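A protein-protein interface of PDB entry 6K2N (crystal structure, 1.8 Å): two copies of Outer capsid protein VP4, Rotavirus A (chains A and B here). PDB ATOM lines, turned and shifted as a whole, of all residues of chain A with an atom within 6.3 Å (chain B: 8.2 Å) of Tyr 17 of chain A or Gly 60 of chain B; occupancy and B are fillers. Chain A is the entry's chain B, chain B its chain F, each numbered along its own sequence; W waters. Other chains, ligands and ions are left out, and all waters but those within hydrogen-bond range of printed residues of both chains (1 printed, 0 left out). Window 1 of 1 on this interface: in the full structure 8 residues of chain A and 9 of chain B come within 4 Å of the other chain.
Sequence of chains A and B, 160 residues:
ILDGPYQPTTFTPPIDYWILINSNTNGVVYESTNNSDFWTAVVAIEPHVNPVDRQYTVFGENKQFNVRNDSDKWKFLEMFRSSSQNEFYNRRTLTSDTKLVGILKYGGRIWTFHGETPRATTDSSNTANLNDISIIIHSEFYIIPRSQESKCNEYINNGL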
ATOM      1  N   PRO A  13       0.160  -8.414  13.003  1.00  0.00           N
ATOM      2  CA  PRO A  13      -0.057  -9.372  11.911  1.00  0.00           C
ATOM      3  C   PRO A  13       0.109 -10.803  12.386  1.00  0.00           C
ATOM      4  O   PRO A  13       1.006 -11.105  13.185  1.00  0.00           O
ATOM      5  CB  PRO A  13       1.031  -9.000  10.889  1.00  0.00           C
ATOM      6  CG  PRO A  13       1.387  -7.603  11.210  1.00  0.00           C
ATOM      7  CD  PRO A  13       1.263  -7.486  12.702  1.00  0.00           C
ATOM      8  N   PRO A  14      -0.734 -11.712  11.905  1.00  0.00           N
ATOM      9  CA  PRO A  14      -0.588 -13.122  12.277  1.00  0.00           C
ATOM     10  C   PRO A  14       0.721 -13.702  11.767  1.00  0.00           C
ATOM     11  O   PRO A  14       1.268 -13.272  10.750  1.00  0.00           O
ATOM     12  CB  PRO A  14      -1.788 -13.790  11.599  1.00  0.00           C
ATOM     13  CG  PRO A  14      -2.079 -12.900  10.421  1.00  0.00           C
ATOM     14  CD  PRO A  14      -1.789 -11.501  10.899  1.00  0.00           C
ATOM     15  N   ILE A  15       1.219 -14.706  12.488  1.00  0.00           N
ATOM     16  CA  ILE A  15       2.388 -15.438  12.025  1.00  0.00           C
ATOM     17  C   ILE A  15       2.048 -16.170  10.732  1.00  0.00           C
ATOM     18  O   ILE A  15       0.912 -16.624  10.536  1.00  0.00           O
ATOM     19  CB  ILE A  15       2.862 -16.409  13.124  1.00  0.00           C
ATOM     20  CG1 ILE A  15       3.284 -15.636  14.376  1.00  0.00           C
ATOM     21  CG2 ILE A  15       4.002 -17.286  12.636  1.00  0.00           C
ATOM     22  CD1 ILE A  15       4.497 -14.767  14.174  1.00  0.00           C
ATOM     23  N   ASP A  16       3.031 -16.247   9.826  1.00  0.00           N
ATOM     24  CA  ASP A  16       2.988 -17.091   8.635  1.00  0.00           C
ATOM     25  C   ASP A  16       2.076 -16.525   7.550  1.00  0.00           C
ATOM     26  O   ASP A  16       1.558 -17.277   6.718  1.00  0.00           O
ATOM     27  CB  ASP A  16       2.560 -18.520   9.022  1.00  0.00           C
ATOM     28  CG  ASP A  16       3.014 -19.568   8.020  1.00  0.00           C
ATOM     29  OD1 ASP A  16       2.241 -20.522   7.763  1.00  0.00           O
ATOM     30  OD2 ASP A  16       4.135 -19.443   7.484  1.00  0.00           O
ATOM     31  N   TYR A  17       1.905 -15.202   7.524  1.00  0.00           N
ATOM     32  CA  TYR A  17       1.161 -14.515   6.472  1.00  0.00           C
ATOM     33  C   TYR A  17       1.981 -13.350   5.935  1.00  0.00           C
ATOM     34  O   TYR A  17       2.488 -12.536   6.712  1.00  0.00           O
ATOM     35  CB  TYR A  17      -0.186 -13.985   6.978  1.00  0.00           C
ATOM     36  CG  TYR A  17      -1.241 -15.046   7.157  1.00  0.00           C
ATOM     37  CD1 TYR A  17      -1.466 -15.622   8.400  1.00  0.00           C
ATOM     38  CD2 TYR A  17      -2.015 -15.472   6.082  1.00  0.00           C
ATOM     39  CE1 TYR A  17      -2.439 -16.603   8.568  1.00  0.00           C
ATOM     40  CE2 TYR A  17      -2.982 -16.449   6.239  1.00  0.00           C
ATOM     41  CZ  TYR A  17      -3.192 -17.009   7.483  1.00  0.00           C
ATOM     42  OH  TYR A  17      -4.159 -17.983   7.629  1.00  0.00           O
ATOM     43  N   TRP A  18       2.096 -13.269   4.612  1.00  0.00           N
ATOM     44  CA  TRP A  18       2.620 -12.076   3.957  1.00  0.00           C
ATOM     45  C   TRP A  18       1.589 -10.960   4.010  1.00  0.00           C
ATOM     46  O   TRP A  18       0.429 -11.155   3.627  1.00  0.00           O
ATOM     47  CB  TRP A  18       2.964 -12.373   2.492  1.00  0.00           C
ATOM     48  CG  TRP A  18       4.269 -13.068   2.315  1.00  0.00           C
ATOM     49  CD1 TRP A  18       4.462 -14.400   2.073  1.00  0.00           C
ATOM     50  CD2 TRP A  18       5.568 -12.474   2.367  1.00  0.00           C
ATOM     51  NE1 TRP A  18       5.807 -14.673   1.981  1.00  0.00           N
ATOM     52  CE2 TRP A  18       6.507 -13.509   2.164  1.00  0.00           C
ATOM     53  CE3 TRP A  18       6.032 -11.172   2.581  1.00  0.00           C
ATOM     54  CZ2 TRP A  18       7.880 -13.278   2.154  1.00  0.00           C
ATOM     55  CZ3 TRP A  18       7.398 -10.947   2.579  1.00  0.00           C
ATOM     56  CH2 TRP A  18       8.305 -11.995   2.366  1.00  0.00           C
ATOM     57  N   ILE A  19       2.010  -9.800   4.501  1.00  0.00           N
ATOM     58  CA  ILE A  19       1.276  -8.554   4.333  1.00  0.00           C
ATOM     59  C   ILE A  19       1.828  -7.870   3.090  1.00  0.00           C
ATOM     60  O   ILE A  19       3.024  -7.563   3.027  1.00  0.00           O
ATOM     61  CB  ILE A  19       1.427  -7.649   5.564  1.00  0.00           C
ATOM     62  CG1 ILE A  19       1.156  -8.415   6.866  1.00  0.00           C
ATOM     63  CG2 ILE A  19       0.565  -6.407   5.424  1.00  0.00           C
ATOM     64  CD1 ILE A  19      -0.143  -9.160   6.900  1.00  0.00           C
ATOM     65  N   ILE A 103       5.833  -7.908   3.839  1.00  0.00           N
ATOM     66  CA  ILE A 103       6.430  -8.173   5.151  1.00  0.00           C
ATOM     67  C   ILE A 103       5.787  -9.419   5.748  1.00  0.00           C
ATOM     68  O   ILE A 103       4.563  -9.565   5.732  1.00  0.00           O
ATOM     69  CB  ILE A 103       6.304  -6.956   6.096  1.00  0.00           C
ATOM     70  CG1 ILE A 103       6.977  -7.240   7.446  1.00  0.00           C
ATOM     71  CG2 ILE A 103       4.849  -6.534   6.279  1.00  0.00           C
ATOM     72  CD1 ILE A 103       7.282  -5.978   8.242  1.00  0.00           C
ATOM     73  N   LEU A 104       6.613 -10.324   6.267  1.00  0.00           N
ATOM     74  CA  LEU A 104       6.151 -11.622   6.740  1.00  0.00           C
ATOM     75  C   LEU A 104       6.810 -11.946   8.070  1.00  0.00           C
ATOM     76  O   LEU A 104       8.026 -11.805   8.206  1.00  0.00           O
ATOM     77  CB  LEU A 104       6.475 -12.727   5.725  1.00  0.00           C
ATOM     78  CG  LEU A 104       6.581 -14.148   6.285  1.00  0.00           C
ATOM     79  CD1 LEU A 104       5.186 -14.723   6.554  1.00  0.00           C
ATOM     80  CD2 LEU A 104       7.363 -15.047   5.339  1.00  0.00           C
ATOM     81  N   LYS A 105       6.025 -12.399   9.038  1.00  0.00           N
ATOM     82  CA  LYS A 105       6.561 -12.921  10.288  1.00  0.00           C
ATOM     83  C   LYS A 105       6.635 -14.437  10.175  1.00  0.00           C
ATOM     84  O   LYS A 105       5.598 -15.097  10.030  1.00  0.00           O
ATOM     85  CB  LYS A 105       5.689 -12.496  11.469  1.00  0.00           C
ATOM     86  CG  LYS A 105       5.648 -10.988  11.682  1.00  0.00           C
ATOM     87  CD  LYS A 105       4.427 -10.535  12.484  1.00  0.00           C
ATOM     88  CE  LYS A 105       4.456 -11.046  13.917  1.00  0.00           C
ATOM     89  NZ  LYS A 105       3.367 -10.443  14.744  1.00  0.00           N
ATOM     90  N   TYR A 106       7.851 -14.992  10.216  1.00  0.00           N
ATOM     91  CA  TYR A 106       7.980 -16.434  10.047  1.00  0.00           C
ATOM     92  C   TYR A 106       9.323 -16.920  10.576  1.00  0.00           C
ATOM     93  O   TYR A 106      10.343 -16.251  10.405  1.00  0.00           O
ATOM     94  CB  TYR A 106       7.839 -16.845   8.580  1.00  0.00           C
ATOM     95  CG  TYR A 106       8.043 -18.325   8.377  1.00  0.00           C
ATOM     96  CD1 TYR A 106       7.040 -19.229   8.697  1.00  0.00           C
ATOM     97  CD2 TYR A 106       9.250 -18.824   7.900  1.00  0.00           C
ATOM     98  CE1 TYR A 106       7.221 -20.584   8.529  1.00  0.00           C
ATOM     99  CE2 TYR A 106       9.440 -20.181   7.728  1.00  0.00           C
ATOM    100  CZ  TYR A 106       8.420 -21.056   8.046  1.00  0.00           C
ATOM    101  OH  TYR A 106       8.590 -22.411   7.880  1.00  0.00           O
ATOM    102  N   ILE A 143      -3.523  -9.905   2.339  1.00  0.00           N
ATOM    103  CA  ILE A 143      -2.961 -10.962   3.173  1.00  0.00           C
ATOM    104  C   ILE A 143      -2.808 -12.207   2.316  1.00  0.00           C
ATOM    105  O   ILE A 143      -3.780 -12.661   1.700  1.00  0.00           O
ATOM    106  CB  ILE A 143      -3.852 -11.274   4.390  1.00  0.00           C
ATOM    107  CG1 ILE A 143      -4.406  -9.990   5.010  1.00  0.00           C
ATOM    108  CG2 ILE A 143      -3.089 -12.121   5.403  1.00  0.00           C
ATOM    109  CD1 ILE A 143      -3.383  -9.136   5.657  1.00  0.00           C
ATOM    110  N   ILE A 144      -1.605 -12.774   2.297  1.00  0.00           N
ATOM    111  CA  ILE A 144      -1.336 -13.959   1.482  1.00  0.00           C
ATOM    112  C   ILE A 144      -0.698 -15.023   2.367  1.00  0.00           C
ATOM    113  O   ILE A 144       0.296 -14.738   3.041  1.00  0.00           O
ATOM    114  CB  ILE A 144      -0.436 -13.617   0.281  1.00  0.00           C
ATOM    115  CG1 ILE A 144      -1.101 -12.560  -0.603  1.00  0.00           C
ATOM    116  CG2 ILE A 144      -0.124 -14.866  -0.537  1.00  0.00           C
ATOM    117  CD1 ILE A 144      -0.236 -12.074  -1.760  1.00  0.00           C
ATOM    118  N   PRO A 145      -1.209 -16.253   2.402  1.00  0.00           N
ATOM    119  CA  PRO A 145      -0.552 -17.284   3.215  1.00  0.00           C
ATOM    120  C   PRO A 145       0.834 -17.600   2.677  1.00  0.00           C
ATOM    121  O   PRO A 145       1.082 -17.545   1.471  1.00  0.00           O
ATOM    122  CB  PRO A 145      -1.485 -18.491   3.083  1.00  0.00           C
ATOM    123  CG  PRO A 145      -2.177 -18.275   1.767  1.00  0.00           C
ATOM    124  CD  PRO A 145      -2.353 -16.789   1.643  1.00  0.00           C
ATOM    125  N   ARG A 146       1.750 -17.924   3.595  1.00  0.00           N
ATOM    126  CA  ARG A 146       3.110 -18.259   3.184  1.00  0.00           C
ATOM    127  C   ARG A 146       3.125 -19.460   2.250  1.00  0.00           C
ATOM    128  O   ARG A 146       4.008 -19.568   1.390  1.00  0.00           O
ATOM    129  CB  ARG A 146       3.993 -18.527   4.401  1.00  0.00           C
ATOM    130  CG  ARG A 146       5.486 -18.490   4.078  1.00  0.00           C
ATOM    131  CD  ARG A 146       6.337 -18.864   5.278  1.00  0.00           C
ATOM    132  NE  ARG A 146       6.454 -20.311   5.420  1.00  0.00           N
ATOM    133  CZ  ARG A 146       7.469 -21.029   4.952  1.00  0.00           C
ATOM    134  NH1 ARG A 146       8.469 -20.436   4.312  1.00  0.00           N
ATOM    135  NH2 ARG A 146       7.488 -22.342   5.128  1.00  0.00           N
ATOM    136  N   SER A 147       2.143 -20.355   2.391  1.00  0.00           N
ATOM    137  CA  SER A 147       1.974 -21.464   1.461  1.00  0.00           C
ATOM    138  C   SER A 147       1.839 -20.997   0.015  1.00  0.00           C
ATOM    139  O   SER A 147       2.030 -21.802  -0.902  1.00  0.00           O
ATOM    140  CB  SER A 147       0.746 -22.283   1.854  1.00  0.00           C
ATOM    141  OG  SER A 147      -0.435 -21.523   1.668  1.00  0.00           O
ATOM    142  N   GLN A 148       1.499 -19.727  -0.214  1.00  0.00           N
ATOM    143  CA  GLN A 148       1.399 -19.179  -1.562  1.00  0.00           C
ATOM    144  C   GLN A 148       2.403 -18.051  -1.787  1.00  0.00           C
ATOM    145  O   GLN A 148       2.145 -17.122  -2.559  1.00  0.00           O
ATOM    146  CB  GLN A 148      -0.023 -18.696  -1.851  1.00  0.00           C
ATOM    147  CG  GLN A 148      -1.105 -19.699  -1.468  1.00  0.00           C
ATOM    148  CD  GLN A 148      -2.500 -19.135  -1.635  1.00  0.00           C
ATOM    149  OE1 GLN A 148      -3.492 -19.861  -1.544  1.00  0.00           O
ATOM    150  NE2 GLN A 148      -2.585 -17.831  -1.876  1.00  0.00           N
ATOM    151  N   THR B  10      -8.600  -8.945  11.373  1.00  0.00           N
ATOM    152  CA  THR B  10      -7.722  -9.642  12.305  1.00  0.00           C
ATOM    153  C   THR B  10      -7.540  -8.751  13.520  1.00  0.00           C
ATOM    154  O   THR B  10      -7.120  -7.597  13.382  1.00  0.00           O
ATOM    155  CB  THR B  10      -6.364  -9.946  11.669  1.00  0.00           C
ATOM    156  OG1 THR B  10      -6.548 -10.750  10.503  1.00  0.00           O
ATOM    157  CG2 THR B  10      -5.457 -10.678  12.662  1.00  0.00           C
ATOM    158  N   VAL B  28     -13.049 -21.482   5.624  1.00  0.00           N
ATOM    159  CA  VAL B  28     -12.613 -21.221   6.992  1.00  0.00           C
ATOM    160  C   VAL B  28     -13.415 -20.044   7.533  1.00  0.00           C
ATOM    161  O   VAL B  28     -13.407 -18.958   6.947  1.00  0.00           O
ATOM    162  CB  VAL B  28     -11.105 -20.941   7.046  1.00  0.00           C
ATOM    163  CG1 VAL B  28     -10.667 -20.616   8.470  1.00  0.00           C
ATOM    164  CG2 VAL B  28     -10.321 -22.130   6.499  1.00  0.00           C
ATOM    165  N   TYR B  30     -13.108 -18.797  10.845  1.00  0.00           N
ATOM    166  CA  TYR B  30     -12.144 -17.998  11.586  1.00  0.00           C
ATOM    167  C   TYR B  30     -10.958 -18.874  11.961  1.00  0.00           C
ATOM    168  O   TYR B  30     -11.053 -20.105  11.989  1.00  0.00           O
ATOM    169  CB  TYR B  30     -12.757 -17.361  12.848  1.00  0.00           C
ATOM    170  CG  TYR B  30     -13.063 -18.319  13.992  1.00  0.00           C
ATOM    171  CD1 TYR B  30     -14.361 -18.771  14.214  1.00  0.00           C
ATOM    172  CD2 TYR B  30     -12.066 -18.741  14.869  1.00  0.00           C
ATOM    173  CE1 TYR B  30     -14.655 -19.625  15.264  1.00  0.00           C
ATOM    174  CE2 TYR B  30     -12.349 -19.601  15.915  1.00  0.00           C
ATOM    175  CZ  TYR B  30     -13.647 -20.038  16.108  1.00  0.00           C
ATOM    176  OH  TYR B  30     -13.937 -20.891  17.147  1.00  0.00           O
ATOM    177  N   GLU B  31      -9.843 -18.208  12.259  1.00  0.00           N
ATOM    178  CA  GLU B  31      -8.627 -18.838  12.770  1.00  0.00           C
ATOM    179  C   GLU B  31      -8.218 -18.105  14.033  1.00  0.00           C
ATOM    180  O   GLU B  31      -8.128 -16.877  14.026  1.00  0.00           O
ATOM    181  CB  GLU B  31      -7.468 -18.760  11.768  1.00  0.00           C
ATOM    182  CG  GLU B  31      -7.741 -19.356  10.416  1.00  0.00           C
ATOM    183  CD  GLU B  31      -6.808 -18.799   9.368  1.00  0.00           C
ATOM    184  OE1 GLU B  31      -7.229 -17.894   8.608  1.00  0.00           O
ATOM    185  OE2 GLU B  31      -5.649 -19.251   9.314  1.00  0.00           O
ATOM    186  N   THR B  33      -5.476 -18.047  17.501  1.00  0.00           N
ATOM    187  CA  THR B  33      -4.295 -18.618  18.149  1.00  0.00           C
ATOM    188  C   THR B  33      -3.614 -17.587  19.037  1.00  0.00           C
ATOM    189  O   THR B  33      -3.755 -16.374  18.848  1.00  0.00           O
ATOM    190  CB  THR B  33      -3.289 -19.172  17.121  1.00  0.00           C
ATOM    191  OG1 THR B  33      -2.244 -19.898  17.796  1.00  0.00           O
ATOM    192  CG2 THR B  33      -2.670 -18.050  16.316  1.00  0.00           C
ATOM    193  N   TYR B  56      -7.765 -26.729   3.148  1.00  0.00           N
ATOM    194  CA  TYR B  56      -8.012 -25.405   3.697  1.00  0.00           C
ATOM    195  C   TYR B  56      -6.689 -24.731   4.023  1.00  0.00           C
ATOM    196  O   TYR B  56      -5.705 -25.385   4.374  1.00  0.00           O
ATOM    197  CB  TYR B  56      -8.873 -25.459   4.967  1.00  0.00           C
ATOM    198  CG  TYR B  56     -10.181 -26.213   4.812  1.00  0.00           C
ATOM    199  CD1 TYR B  56     -11.337 -25.558   4.419  1.00  0.00           C
ATOM    200  CD2 TYR B  56     -10.255 -27.579   5.072  1.00  0.00           C
ATOM    201  CE1 TYR B  56     -12.532 -26.238   4.286  1.00  0.00           C
ATOM    202  CE2 TYR B  56     -11.441 -28.266   4.943  1.00  0.00           C
ATOM    203  CZ  TYR B  56     -12.581 -27.589   4.546  1.00  0.00           C
ATOM    204  OH  TYR B  56     -13.780 -28.251   4.414  1.00  0.00           O
ATOM    205  N   THR B  57      -6.676 -23.412   3.924  1.00  0.00           N
ATOM    206  CA  THR B  57      -5.527 -22.618   4.335  1.00  0.00           C
ATOM    207  C   THR B  57      -5.779 -22.135   5.757  1.00  0.00           C
ATOM    208  O   THR B  57      -6.685 -21.329   5.993  1.00  0.00           O
ATOM    209  CB  THR B  57      -5.296 -21.448   3.389  1.00  0.00           C
ATOM    210  OG1 THR B  57      -4.917 -21.952   2.106  1.00  0.00           O
ATOM    211  CG2 THR B  57      -4.188 -20.568   3.924  1.00  0.00           C
ATOM    212  N   VAL B  58      -4.997 -22.643   6.703  1.00  0.00           N
ATOM    213  CA  VAL B  58      -5.128 -22.265   8.102  1.00  0.00           C
ATOM    214  C   VAL B  58      -3.754 -21.903   8.644  1.00  0.00           C
ATOM    215  O   VAL B  58      -2.777 -22.640   8.439  1.00  0.00           O
ATOM    216  CB  VAL B  58      -5.792 -23.374   8.943  1.00  0.00           C
ATOM    217  CG1 VAL B  58      -7.241 -23.569   8.497  1.00  0.00           C
ATOM    218  CG2 VAL B  58      -5.028 -24.675   8.831  1.00  0.00           C
ATOM    219  N   PHE B  59      -3.681 -20.748   9.310  1.00  0.00           N
ATOM    220  CA  PHE B  59      -2.447 -20.254   9.914  1.00  0.00           C
ATOM    221  C   PHE B  59      -1.313 -20.227   8.893  1.00  0.00           C
ATOM    222  O   PHE B  59      -0.162 -20.542   9.196  1.00  0.00           O
ATOM    223  CB  PHE B  59      -2.090 -21.081  11.149  1.00  0.00           C
ATOM    224  CG  PHE B  59      -3.209 -21.154  12.148  1.00  0.00           C
ATOM    225  CD1 PHE B  59      -3.513 -20.061  12.946  1.00  0.00           C
ATOM    226  CD2 PHE B  59      -3.987 -22.295  12.255  1.00  0.00           C
ATOM    227  CE1 PHE B  59      -4.554 -20.117  13.860  1.00  0.00           C
ATOM    228  CE2 PHE B  59      -5.033 -22.355  13.161  1.00  0.00           C
ATOM    229  CZ  PHE B  59      -5.319 -21.264  13.960  1.00  0.00           C
ATOM    230  N   GLY B  60      -1.656 -19.855   7.662  1.00  0.00           N
ATOM    231  CA  GLY B  60      -0.689 -19.706   6.599  1.00  0.00           C
ATOM    232  C   GLY B  60      -0.257 -20.987   5.919  1.00  0.00           C
ATOM    233  O   GLY B  60       0.641 -20.937   5.070  1.00  0.00           O
ATOM    234  N   GLU B  61      -0.858 -22.130   6.250  1.00  0.00           N
ATOM    235  CA  GLU B  61      -0.427 -23.405   5.696  1.00  0.00           C
ATOM    236  C   GLU B  61      -1.582 -24.141   5.031  1.00  0.00           C
ATOM    237  O   GLU B  61      -2.753 -23.948   5.376  1.00  0.00           O
ATOM    238  CB  GLU B  61       0.188 -24.305   6.782  1.00  0.00           C
ATOM    239  CG  GLU B  61       1.466 -23.761   7.400  1.00  0.00           C
ATOM    240  CD  GLU B  61       1.926 -24.583   8.591  1.00  0.00           C
ATOM    241  OE1 GLU B  61       1.228 -25.554   8.951  1.00  0.00           O
ATOM    242  OE2 GLU B  61       2.982 -24.256   9.172  1.00  0.00           O
ATOM    243  N   ASN B  62      -1.231 -24.998   4.074  1.00  0.00           N
ATOM    244  CA  ASN B  62      -2.179 -25.893   3.429  1.00  0.00           C
ATOM    245  C   ASN B  62      -2.383 -27.123   4.303  1.00  0.00           C
ATOM    246  O   ASN B  62      -1.420 -27.825   4.624  1.00  0.00           O
ATOM    247  CB  ASN B  62      -1.659 -26.305   2.053  1.00  0.00           C
ATOM    248  CG  ASN B  62      -2.014 -25.319   0.970  1.00  0.00           C
ATOM    249  OD1 ASN B  62      -1.761 -25.570  -0.205  1.00  0.00           O
ATOM    250  ND2 ASN B  62      -2.604 -24.186   1.354  1.00  0.00           N
ATOM    251  N   LYS B  63      -3.627 -27.390   4.690  1.00  0.00           N
ATOM    252  CA  LYS B  63      -3.949 -28.556   5.494  1.00  0.00           C
ATOM    253  C   LYS B  63      -5.103 -29.302   4.844  1.00  0.00           C
ATOM    254  O   LYS B  63      -5.962 -28.703   4.196  1.00  0.00           O
ATOM    255  CB  LYS B  63      -4.321 -28.168   6.930  1.00  0.00           C
ATOM    256  CG  LYS B  63      -3.173 -27.558   7.719  1.00  0.00           C
ATOM    257  CD  LYS B  63      -2.128 -28.611   8.093  1.00  0.00           C
ATOM    258  CE  LYS B  63      -0.988 -27.992   8.890  1.00  0.00           C
ATOM    259  NZ  LYS B  63       0.059 -28.987   9.255  1.00  0.00           N
ATOM    260  N   ARG B  81      -5.376 -27.742  17.695  1.00  0.00           N
ATOM    261  CA  ARG B  81      -4.091 -28.304  18.098  1.00  0.00           C
ATOM    262  C   ARG B  81      -3.519 -27.449  19.221  1.00  0.00           C
ATOM    263  O   ARG B  81      -3.735 -26.234  19.268  1.00  0.00           O
ATOM    264  CB  ARG B  81      -3.103 -28.398  16.925  1.00  0.00           C
ATOM    265  CG  ARG B  81      -2.432 -27.086  16.565  1.00  0.00           C
ATOM    266  CD  ARG B  81      -1.625 -27.186  15.282  1.00  0.00           C
ATOM    267  NE  ARG B  81      -1.059 -25.891  14.915  1.00  0.00           N
ATOM    268  CZ  ARG B  81      -0.381 -25.654  13.796  1.00  0.00           C
ATOM    269  NH1 ARG B  81      -0.176 -26.629  12.922  1.00  0.00           N
ATOM    270  NH2 ARG B  81       0.095 -24.441  13.552  1.00  0.00           N
ATOM    271  N   ILE B 136      -8.453 -14.197  13.226  1.00  0.00           N
ATOM    272  CA  ILE B 136      -8.742 -13.769  11.863  1.00  0.00           C
ATOM    273  C   ILE B 136     -10.155 -14.224  11.546  1.00  0.00           C
ATOM    274  O   ILE B 136     -10.439 -15.430  11.556  1.00  0.00           O
ATOM    275  CB  ILE B 136      -7.742 -14.367  10.859  1.00  0.00           C
ATOM    276  CG1 ILE B 136      -6.303 -14.093  11.293  1.00  0.00           C
ATOM    277  CG2 ILE B 136      -8.004 -13.828   9.452  1.00  0.00           C
ATOM    278  CD1 ILE B 136      -5.276 -14.695  10.347  1.00  0.00           C
ATOM    279  N   HIS B 138     -13.311 -14.219   8.824  1.00  0.00           N
ATOM    280  CA  HIS B 138     -13.483 -14.197   7.377  1.00  0.00           C
ATOM    281  C   HIS B 138     -14.892 -13.810   6.937  1.00  0.00           C
ATOM    282  O   HIS B 138     -15.202 -13.907   5.747  1.00  0.00           O
ATOM    283  CB  HIS B 138     -13.122 -15.563   6.788  1.00  0.00           C
ATOM    284  CG  HIS B 138     -11.676 -15.917   6.925  1.00  0.00           C
ATOM    285  ND1 HIS B 138     -10.664 -15.103   6.462  1.00  0.00           N
ATOM    286  CD2 HIS B 138     -11.069 -16.998   7.469  1.00  0.00           C
ATOM    287  CE1 HIS B 138      -9.496 -15.669   6.715  1.00  0.00           C
ATOM    288  NE2 HIS B 138      -9.716 -16.821   7.324  1.00  0.00           N
HETATM  289  O   HOH W   1      -6.591 -15.863   6.727  1.00  0.00           O
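OH of Tyr 17 of chain A sits at hydrogen-bond distance from OE2 of Glu 31 of chain B (2.6 Å). The side-chain hydroxyl of Tyr 17 of chain A lies within hydrogen-bond range of the backbone NH of Phe 59 of chain B (3.3 Å). The backbone NH (N) of Gly 60 of chain B is in hydrogen-bond range of the side-chain hydroxyl (OH) of Tyr 17 of chain A, at 3.1 Å. The backbone NH (N) of Ser 147 of chain A lies within hydrogen-bond range of the backbone carbonyl oxygen (O) of Gly 60 of chain B. OG of Ser 147 of chain A sits at hydrogen-bond distance from ND2 of Asn 62 of chain B. The side-chain carboxylate of Asp 16 of chain A lies close to the backbone carbonyl oxygen of Phe 59 of chain B, at 2.8 Å. OD1 of Asp 16 of chain A lies close to O of Gly 60 of chain B (3.2 Å).
OD2 of Asp 16 of chain A lies within salt-bridge range of NE of Arg 146 of chain A (3.2 Å). OH of Tyr 106 of chain A sits at hydrogen-bond distance from NH2 of Arg 146 of chain A (3.0 Å). The side-chain carboxylate (OE2) of Glu 31 of chain B is in hydrogen-bond range of the backbone NH (N) of Phe 59 of chain B, 2.5 Å away. The side-chain carboxylate (OE1) of Glu 31 of chain B sits at hydrogen-bond distance from a ring nitrogen (NE2) of His 138 of chain B, 3.0 Å away. OG1 of Thr 57 of chain B sits at hydrogen-bond distance from ND2 of Asn 62 of chain B (3.3 Å). The side-chain carboxylate of Glu 61 of chain B lies within salt-bridge range of the side-chain amino group of Lys 63 of chain B (3.6 Å).
Among the printed residues, pairs that only touch across the chains: Asp 16 of chain A with Glu 61 of chain B (3.4 Å), Pro 145 of chain A with Thr 57 of chain B (3.5 Å), Arg 146 of chain A with Gly 60 of chain B (3.5 Å), Pro 14 of chain A with Ile 136 of chain B (3.7 Å), Pro 145 of chain A with Gly 60 of chain B (3.8 Å) and Tyr 17 of chain A with Ile 136 of chain B (3.9 Å).
Of the printed residues of chain B, Tyr 17 of chain A touches Glu 31 (2.6 Å), Phe 59 (3.3 Å), Gly 60 (3.1 Å) and Ile 136 (3.9 Å). Printed residues of chain B within 4 Å of Asp 16 of chain A: Phe 59 (2.8 Å), Gly 60 (3.1 Å) and Glu 61 (3.4 Å). Printed residues of chain A within 4 Å of Ile 136 of chain B: Pro 14 and Tyr 17. Of the printed residues of chain A, Glu 31 of chain B touches Tyr 17. Of the printed residues of chain A, Asn 62 of chain B touches Ser 147 (3.4 Å). Ile 103 of chain A touches none of the printed residues of chain B. The nearest residue of chain B that does not touch Tyr 17 of chain A is Val 58 of chain B (4.1 Å). The nearest residue of chain A that does not touch Gly 60 of chain B is Ile 15 of chain A (5.0 Å).
Of the 17 printed residues of chain A, 6 touch a printed residue of chain B. Hydrophobic or aromatic side chains of chain A that line the printed part of chain B: Pro 14, Tyr 17 and Pro 145. Of the 16 printed residues of chain B, 7 touch a printed residue of chain A. Printed residues of chain B that touch a printed residue of chain A: Glu 31, Thr 57, Phe 59, Gly 60, Glu 61, Asn 62 and Ile 136. Among the printed residues, 13 pairs touch across the chains. Among the printed residues, no Asp or Glu carboxylate lies within 4 Å of a Lys or Arg side-chain nitrogen of the other chain.
No position is printed for both chains. Of the 13 pairs that touch across the chains among the printed residues, none has its exchanged pair printed and touching as well.
Water W1 lies within hydrogen-bond range of the side-chain carboxylate of Glu 31 of chain B (2.8 Å), a ring nitrogen (NE2) of His 138 of chain B (3.3 Å) and the side-chain hydroxyl of Tyr 17 of chain A (3.4 Å).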
